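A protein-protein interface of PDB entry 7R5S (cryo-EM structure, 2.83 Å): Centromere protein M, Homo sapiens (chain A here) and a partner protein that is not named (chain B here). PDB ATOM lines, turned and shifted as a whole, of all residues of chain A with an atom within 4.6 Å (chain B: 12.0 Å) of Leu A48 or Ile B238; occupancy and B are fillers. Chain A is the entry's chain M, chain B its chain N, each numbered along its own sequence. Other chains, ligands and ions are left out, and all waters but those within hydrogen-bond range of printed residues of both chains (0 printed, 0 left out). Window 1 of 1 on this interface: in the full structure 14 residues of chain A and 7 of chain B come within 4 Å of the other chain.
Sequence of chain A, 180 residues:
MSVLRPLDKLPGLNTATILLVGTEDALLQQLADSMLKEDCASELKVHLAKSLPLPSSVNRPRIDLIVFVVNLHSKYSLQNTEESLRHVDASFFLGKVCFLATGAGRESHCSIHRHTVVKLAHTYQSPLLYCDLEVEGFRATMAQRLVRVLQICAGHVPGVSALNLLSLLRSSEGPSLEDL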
ATOM      1  N   LEU A  19      -8.908  23.876  12.005  1.00  0.00           N
ATOM      2  CA  LEU A  19      -8.761  22.606  12.706  1.00  0.00           C
ATOM      3  C   LEU A  19     -10.134  21.980  12.895  1.00  0.00           C
ATOM      4  O   LEU A  19     -11.067  22.652  13.343  1.00  0.00           O
ATOM      5  CB  LEU A  19      -8.074  22.801  14.062  1.00  0.00           C
ATOM      6  CG  LEU A  19      -7.967  21.573  14.969  1.00  0.00           C
ATOM      7  CD1 LEU A  19      -7.086  20.511  14.336  1.00  0.00           C
ATOM      8  CD2 LEU A  19      -7.438  21.963  16.339  1.00  0.00           C
ATOM      9  N   LEU A  20     -10.253  20.697  12.558  1.00  0.00           N
ATOM     10  CA  LEU A  20     -11.508  19.962  12.663  1.00  0.00           C
ATOM     11  C   LEU A  20     -11.321  18.803  13.630  1.00  0.00           C
ATOM     12  O   LEU A  20     -10.482  17.926  13.397  1.00  0.00           O
ATOM     13  CB  LEU A  20     -11.961  19.452  11.294  1.00  0.00           C
ATOM     14  CG  LEU A  20     -12.155  20.504  10.200  1.00  0.00           C
ATOM     15  CD1 LEU A  20     -12.534  19.846   8.885  1.00  0.00           C
ATOM     16  CD2 LEU A  20     -13.203  21.523  10.614  1.00  0.00           C
ATOM     17  N   ASP A  25     -13.847   9.938  11.012  1.00  0.00           N
ATOM     18  CA  ASP A  25     -12.777  10.455  10.166  1.00  0.00           C
ATOM     19  C   ASP A  25     -13.215  10.625   8.717  1.00  0.00           C
ATOM     20  O   ASP A  25     -12.717  11.522   8.026  1.00  0.00           O
ATOM     21  CB  ASP A  25     -11.559   9.534  10.239  1.00  0.00           C
ATOM     22  CG  ASP A  25     -10.350  10.112   9.531  1.00  0.00           C
ATOM     23  OD1 ASP A  25      -9.754  11.074  10.059  1.00  0.00           O
ATOM     24  OD2 ASP A  25      -9.995   9.605   8.446  1.00  0.00           O
ATOM     25  N   LEU A  28     -14.920  13.992   8.295  1.00  0.00           N
ATOM     26  CA  LEU A  28     -13.935  15.067   8.332  1.00  0.00           C
ATOM     27  C   LEU A  28     -13.148  15.139   7.030  1.00  0.00           C
ATOM     28  O   LEU A  28     -12.872  16.232   6.521  1.00  0.00           O
ATOM     29  CB  LEU A  28     -12.991  14.876   9.519  1.00  0.00           C
ATOM     30  CG  LEU A  28     -13.633  14.883  10.907  1.00  0.00           C
ATOM     31  CD1 LEU A  28     -12.575  14.728  11.988  1.00  0.00           C
ATOM     32  CD2 LEU A  28     -14.443  16.151  11.121  1.00  0.00           C
ATOM     33  N   GLN A  29     -12.779  13.983   6.472  1.00  0.00           N
ATOM     34  CA  GLN A  29     -12.066  13.972   5.199  1.00  0.00           C
ATOM     35  C   GLN A  29     -12.929  14.543   4.079  1.00  0.00           C
ATOM     36  O   GLN A  29     -12.450  15.331   3.254  1.00  0.00           O
ATOM     37  CB  GLN A  29     -11.619  12.551   4.860  1.00  0.00           C
ATOM     38  CG  GLN A  29     -10.772  12.447   3.603  1.00  0.00           C
ATOM     39  CD  GLN A  29      -9.366  12.975   3.800  1.00  0.00           C
ATOM     40  OE1 GLN A  29      -8.881  13.076   4.927  1.00  0.00           O
ATOM     41  NE2 GLN A  29      -8.702  13.316   2.701  1.00  0.00           N
ATOM     42  N   VAL A  46      -5.872  22.736   6.317  1.00  0.00           N
ATOM     43  CA  VAL A  46      -6.847  22.019   7.129  1.00  0.00           C
ATOM     44  C   VAL A  46      -6.115  20.961   7.942  1.00  0.00           C
ATOM     45  O   VAL A  46      -5.327  20.184   7.391  1.00  0.00           O
ATOM     46  CB  VAL A  46      -7.945  21.375   6.263  1.00  0.00           C
ATOM     47  CG1 VAL A  46      -8.968  20.671   7.139  1.00  0.00           C
ATOM     48  CG2 VAL A  46      -8.617  22.422   5.388  1.00  0.00           C
ATOM     49  N   HIS A  47      -6.376  20.933   9.246  1.00  0.00           N
ATOM     50  CA  HIS A  47      -5.844  19.916  10.140  1.00  0.00           C
ATOM     51  C   HIS A  47      -6.997  19.099  10.702  1.00  0.00           C
ATOM     52  O   HIS A  47      -8.073  19.637  10.978  1.00  0.00           O
ATOM     53  CB  HIS A  47      -5.038  20.545  11.281  1.00  0.00           C
ATOM     54  CG  HIS A  47      -3.759  21.183  10.838  1.00  0.00           C
ATOM     55  ND1 HIS A  47      -2.531  20.826  11.354  1.00  0.00           N
ATOM     56  CD2 HIS A  47      -3.515  22.156   9.929  1.00  0.00           C
ATOM     57  CE1 HIS A  47      -1.588  21.552  10.781  1.00  0.00           C
ATOM     58  NE2 HIS A  47      -2.158  22.367   9.912  1.00  0.00           N
ATOM     59  N   LEU A  48      -6.772  17.798  10.860  1.00  0.00           N
ATOM     60  CA  LEU A  48      -7.779  16.879  11.371  1.00  0.00           C
ATOM     61  C   LEU A  48      -7.294  16.263  12.674  1.00  0.00           C
ATOM     62  O   LEU A  48      -6.116  15.918  12.807  1.00  0.00           O
ATOM     63  CB  LEU A  48      -8.087  15.777  10.353  1.00  0.00           C
ATOM     64  CG  LEU A  48      -8.567  16.237   8.976  1.00  0.00           C
ATOM     65  CD1 LEU A  48      -8.791  15.044   8.062  1.00  0.00           C
ATOM     66  CD2 LEU A  48      -9.834  17.064   9.100  1.00  0.00           C
ATOM     67  N   ALA A  49      -8.205  16.123  13.635  1.00  0.00           N
ATOM     68  CA  ALA A  49      -7.857  15.539  14.921  1.00  0.00           C
ATOM     69  C   ALA A  49      -9.063  14.800  15.478  1.00  0.00           C
ATOM     70  O   ALA A  49     -10.206  15.049  15.089  1.00  0.00           O
ATOM     71  CB  ALA A  49      -7.376  16.603  15.912  1.00  0.00           C
ATOM     72  N   MET B 233      -0.882  13.508  -2.590  1.00  0.00           N
ATOM     73  CA  MET B 233      -2.339  13.484  -2.648  1.00  0.00           C
ATOM     74  C   MET B 233      -2.942  14.519  -1.703  1.00  0.00           C
ATOM     75  O   MET B 233      -3.204  14.225  -0.537  1.00  0.00           O
ATOM     76  CB  MET B 233      -2.866  12.089  -2.305  1.00  0.00           C
ATOM     77  N   ASP B 234      -3.158  15.729  -2.223  1.00  0.00           N
ATOM     78  CA  ASP B 234      -3.739  16.842  -1.469  1.00  0.00           C
ATOM     79  C   ASP B 234      -2.899  17.148  -0.225  1.00  0.00           C
ATOM     80  O   ASP B 234      -3.329  16.989   0.919  1.00  0.00           O
ATOM     81  CB  ASP B 234      -5.200  16.552  -1.104  1.00  0.00           C
ATOM     82  CG  ASP B 234      -6.076  17.786  -1.190  1.00  0.00           C
ATOM     83  OD1 ASP B 234      -5.549  18.868  -1.520  1.00  0.00           O
ATOM     84  OD2 ASP B 234      -7.292  17.672  -0.930  1.00  0.00           O
ATOM     85  N   SER B 235      -1.669  17.591  -0.493  1.00  0.00           N
ATOM     86  CA  SER B 235      -0.711  17.893   0.565  1.00  0.00           C
ATOM     87  C   SER B 235      -1.174  19.007   1.495  1.00  0.00           C
ATOM     88  O   SER B 235      -0.572  19.189   2.559  1.00  0.00           O
ATOM     89  CB  SER B 235       0.640  18.265  -0.047  1.00  0.00           C
ATOM     90  OG  SER B 235       0.477  19.160  -1.133  1.00  0.00           O
ATOM     91  N   ARG B 236      -2.216  19.758   1.127  1.00  0.00           N
ATOM     92  CA  ARG B 236      -2.711  20.815   1.999  1.00  0.00           C
ATOM     93  C   ARG B 236      -3.406  20.268   3.239  1.00  0.00           C
ATOM     94  O   ARG B 236      -3.504  20.980   4.243  1.00  0.00           O
ATOM     95  CB  ARG B 236      -3.663  21.731   1.228  1.00  0.00           C
ATOM     96  CG  ARG B 236      -2.972  22.641   0.227  1.00  0.00           C
ATOM     97  CD  ARG B 236      -3.973  23.506  -0.520  1.00  0.00           C
ATOM     98  NE  ARG B 236      -4.800  22.725  -1.436  1.00  0.00           N
ATOM     99  CZ  ARG B 236      -5.755  23.239  -2.203  1.00  0.00           C
ATOM    100  NH1 ARG B 236      -6.010  24.539  -2.166  1.00  0.00           N
ATOM    101  NH2 ARG B 236      -6.456  22.454  -3.008  1.00  0.00           N
ATOM    102  N   ILE B 237      -3.888  19.030   3.194  1.00  0.00           N
ATOM    103  CA  ILE B 237      -4.528  18.399   4.342  1.00  0.00           C
ATOM    104  C   ILE B 237      -3.459  17.727   5.190  1.00  0.00           C
ATOM    105  O   ILE B 237      -2.633  16.964   4.675  1.00  0.00           O
ATOM    106  CB  ILE B 237      -5.593  17.386   3.891  1.00  0.00           C
ATOM    107  CG1 ILE B 237      -6.628  18.061   2.993  1.00  0.00           C
ATOM    108  CG2 ILE B 237      -6.270  16.753   5.097  1.00  0.00           C
ATOM    109  CD1 ILE B 237      -7.714  17.130   2.507  1.00  0.00           C
ATOM    110  N   ILE B 238      -3.475  18.004   6.490  1.00  0.00           N
ATOM    111  CA  ILE B 238      -2.524  17.431   7.436  1.00  0.00           C
ATOM    112  C   ILE B 238      -3.281  16.459   8.329  1.00  0.00           C
ATOM    113  O   ILE B 238      -4.173  16.864   9.083  1.00  0.00           O
ATOM    114  CB  ILE B 238      -1.824  18.516   8.267  1.00  0.00           C
ATOM    115  CG1 ILE B 238      -1.082  19.492   7.353  1.00  0.00           C
ATOM    116  CG2 ILE B 238      -0.865  17.886   9.264  1.00  0.00           C
ATOM    117  CD1 ILE B 238      -0.023  18.839   6.496  1.00  0.00           C
ATOM    118  N   HIS B 239      -2.923  15.180   8.246  1.00  0.00           N
ATOM    119  CA  HIS B 239      -3.572  14.136   9.032  1.00  0.00           C
ATOM    120  C   HIS B 239      -2.788  13.932  10.323  1.00  0.00           C
ATOM    121  O   HIS B 239      -1.675  13.398  10.303  1.00  0.00           O
ATOM    122  CB  HIS B 239      -3.659  12.835   8.239  1.00  0.00           C
ATOM    123  CG  HIS B 239      -4.640  12.878   7.109  1.00  0.00           C
ATOM    124  ND1 HIS B 239      -4.333  13.412   5.877  1.00  0.00           N
ATOM    125  CD2 HIS B 239      -5.921  12.448   7.024  1.00  0.00           C
ATOM    126  CE1 HIS B 239      -5.383  13.312   5.081  1.00  0.00           C
ATOM    127  NE2 HIS B 239      -6.361  12.731   5.754  1.00  0.00           N
ATOM    128  N   GLU B 240      -3.365  14.358  11.439  1.00  0.00           N
ATOM    129  CA  GLU B 240      -2.779  14.092  12.742  1.00  0.00           C
ATOM    130  C   GLU B 240      -3.254  12.737  13.259  1.00  0.00           C
ATOM    131  O   GLU B 240      -4.167  12.118  12.709  1.00  0.00           O
ATOM    132  CB  GLU B 240      -3.129  15.205  13.728  1.00  0.00           C
ATOM    133  CG  GLU B 240      -2.533  16.553  13.363  1.00  0.00           C
ATOM    134  CD  GLU B 240      -2.897  17.639  14.352  1.00  0.00           C
ATOM    135  OE1 GLU B 240      -3.802  17.410  15.182  1.00  0.00           O
ATOM    136  OE2 GLU B 240      -2.276  18.721  14.301  1.00  0.00           O
ATOM    137  N   ASN B 241      -2.611  12.276  14.335  1.00  0.00           N
ATOM    138  CA  ASN B 241      -2.862  10.951  14.901  1.00  0.00           C
ATOM    139  C   ASN B 241      -2.641   9.848  13.871  1.00  0.00           C
ATOM    140  O   ASN B 241      -3.294   8.802  13.914  1.00  0.00           O
ATOM    141  CB  ASN B 241      -4.273  10.850  15.495  1.00  0.00           C
ATOM    142  CG  ASN B 241      -4.575  11.964  16.475  1.00  0.00           C
ATOM    143  OD1 ASN B 241      -5.541  12.707  16.308  1.00  0.00           O
ATOM    144  ND2 ASN B 241      -3.749  12.083  17.507  1.00  0.00           N
ATOM    145  N   ILE B 242      -1.719  10.074  12.933  1.00  0.00           N
ATOM    146  CA  ILE B 242      -1.451   9.079  11.901  1.00  0.00           C
ATOM    147  C   ILE B 242      -0.703   7.886  12.484  1.00  0.00           C
ATOM    148  O   ILE B 242      -0.846   6.754  12.000  1.00  0.00           O
ATOM    149  CB  ILE B 242      -0.685   9.725  10.729  1.00  0.00           C
ATOM    150  CG1 ILE B 242      -0.519   8.736   9.574  1.00  0.00           C
ATOM    151  CG2 ILE B 242       0.665  10.257  11.191  1.00  0.00           C
ATOM    152  CD1 ILE B 242      -1.828   8.298   8.955  1.00  0.00           C
ATOM    153  N   VAL B 243       0.088   8.108  13.535  1.00  0.00           N
ATOM    154  CA  VAL B 243       0.797   7.004  14.173  1.00  0.00           C
ATOM    155  C   VAL B 243      -0.188   6.049  14.835  1.00  0.00           C
ATOM    156  O   VAL B 243      -0.021   4.826  14.775  1.00  0.00           O
ATOM    157  CB  VAL B 243       1.837   7.541  15.175  1.00  0.00           C
ATOM    158  CG1 VAL B 243       3.031   8.119  14.433  1.00  0.00           C
ATOM    159  CG2 VAL B 243       1.216   8.595  16.077  1.00  0.00           C
ATOM    160  N   GLU B 244      -1.240   6.586  15.457  1.00  0.00           N
ATOM    161  CA  GLU B 244      -2.261   5.724  16.044  1.00  0.00           C
ATOM    162  C   GLU B 244      -2.996   4.934  14.969  1.00  0.00           C
ATOM    163  O   GLU B 244      -3.333   3.761  15.172  1.00  0.00           O
ATOM    164  CB  GLU B 244      -3.242   6.558  16.867  1.00  0.00           C
ATOM    165  CG  GLU B 244      -4.152   5.740  17.768  1.00  0.00           C
ATOM    166  CD  GLU B 244      -3.431   5.183  18.980  1.00  0.00           C
ATOM    167  OE1 GLU B 244      -2.321   5.666  19.289  1.00  0.00           O
ATOM    168  OE2 GLU B 244      -3.973   4.261  19.624  1.00  0.00           O
ATOM    169  N   LYS B 245      -3.241   5.555  13.813  1.00  0.00           N
ATOM    170  CA  LYS B 245      -3.914   4.858  12.722  1.00  0.00           C
ATOM    171  C   LYS B 245      -3.057   3.717  12.188  1.00  0.00           C
ATOM    172  O   LYS B 245      -3.548   2.600  11.982  1.00  0.00           O
ATOM    173  CB  LYS B 245      -4.264   5.843  11.607  1.00  0.00           C
ATOM    174  CG  LYS B 245      -5.222   6.942  12.032  1.00  0.00           C
ATOM    175  CD  LYS B 245      -5.539   7.880  10.878  1.00  0.00           C
ATOM    176  CE  LYS B 245      -6.233   7.144   9.745  1.00  0.00           C
ATOM    177  NZ  LYS B 245      -6.566   8.054   8.614  1.00  0.00           N
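O of His A47 lies within hydrogen-bond range of N of Leu A20, at 2.9 Å.
The backbone carbonyl oxygen of Leu A20 sits at hydrogen-bond distance from the backbone NH of Ala A49 (2.9 Å).
OD1 of Asp B234 lies within salt-bridge range of NE of Arg B236 (3.9 Å).
Ile B238 touches just these residues of chain A: Val A46, His A47 and Leu A48.
Leu A20 touches none of the printed residues of chain B.
Of chain B, only Arg B236 (3.6 Å), Ile B237 (3.6 Å) and Ile B238 (3.0 Å) come within 4 Å of Val A46.
Of chain B, only Ile B238 (3.6 Å) and Glu B240 (3.6 Å) come within 4 Å of His A47.
Printed residues of chain B within 4 Å of Ala A49: Glu B240 (3.7 Å) and Asn B241 (3.9 Å).
Of the printed residues of chain A, Ile B237 touches Gln A29 (3.9 Å) and Val A46 (3.6 Å).
Of the printed residues of chain A, Glu B240 touches His A47, Leu A48 and Ala A49.
Of the printed residues of chain A, Arg B236 touches Val A46 (3.6 Å).
Printed residues of chain A within 4 Å of His B239: Gln A29 (2.7 Å).
Ser B235 touches none of the printed residues of chain A.
Asp B234 touches none of the printed residues of chain A.
The nearest printed residue of chain B that does not touch Leu A48 is His B239 (4.01 Å).
Ile B237 touches Gln A29.
Val A46 touches Arg B236.
Ile B237 touches Val A46.
Ile B238 touches His A47 (O to CA, 3.6 Å).
His A47 touches Glu B240.
Ala A49 touches Glu B240 (CB to OE1, 3.7 Å).
Asn B241 touches Ala A49.
Hydrophobic or aromatic side chains of chain B within 4 Å of the printed part of chain A: Ile B237, Ile B238 and His B239.
Along chain A the printed residues that touch a printed residue of chain B span positions 25 to 49.
Among the printed residues, Asp or Glu carboxylates within 4 Å of a Lys or Arg side-chain nitrogen of the other chain: Asp A25 with Lys B245 (3.8 Å).
OE1 of Gln A29 is in hydrogen-bond range of NE2 of His B239, at 2.7 Å.
The backbone carbonyl oxygen of Ile B238 lies within hydrogen-bond range of the backbone NH of Leu A48, at 3.3 Å.
The side-chain carboxylate (OD2) of Asp A25 is in salt-bridge range of the side-chain amino group (NZ) of Lys B245 (3.8 Å).
The backbone NH (N) of Glu B240 sits close to the backbone carbonyl oxygen (O) of Leu A48 (3.4 Å).
O of Val A46 is in hydrogen-bond range of N of Ile B238.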
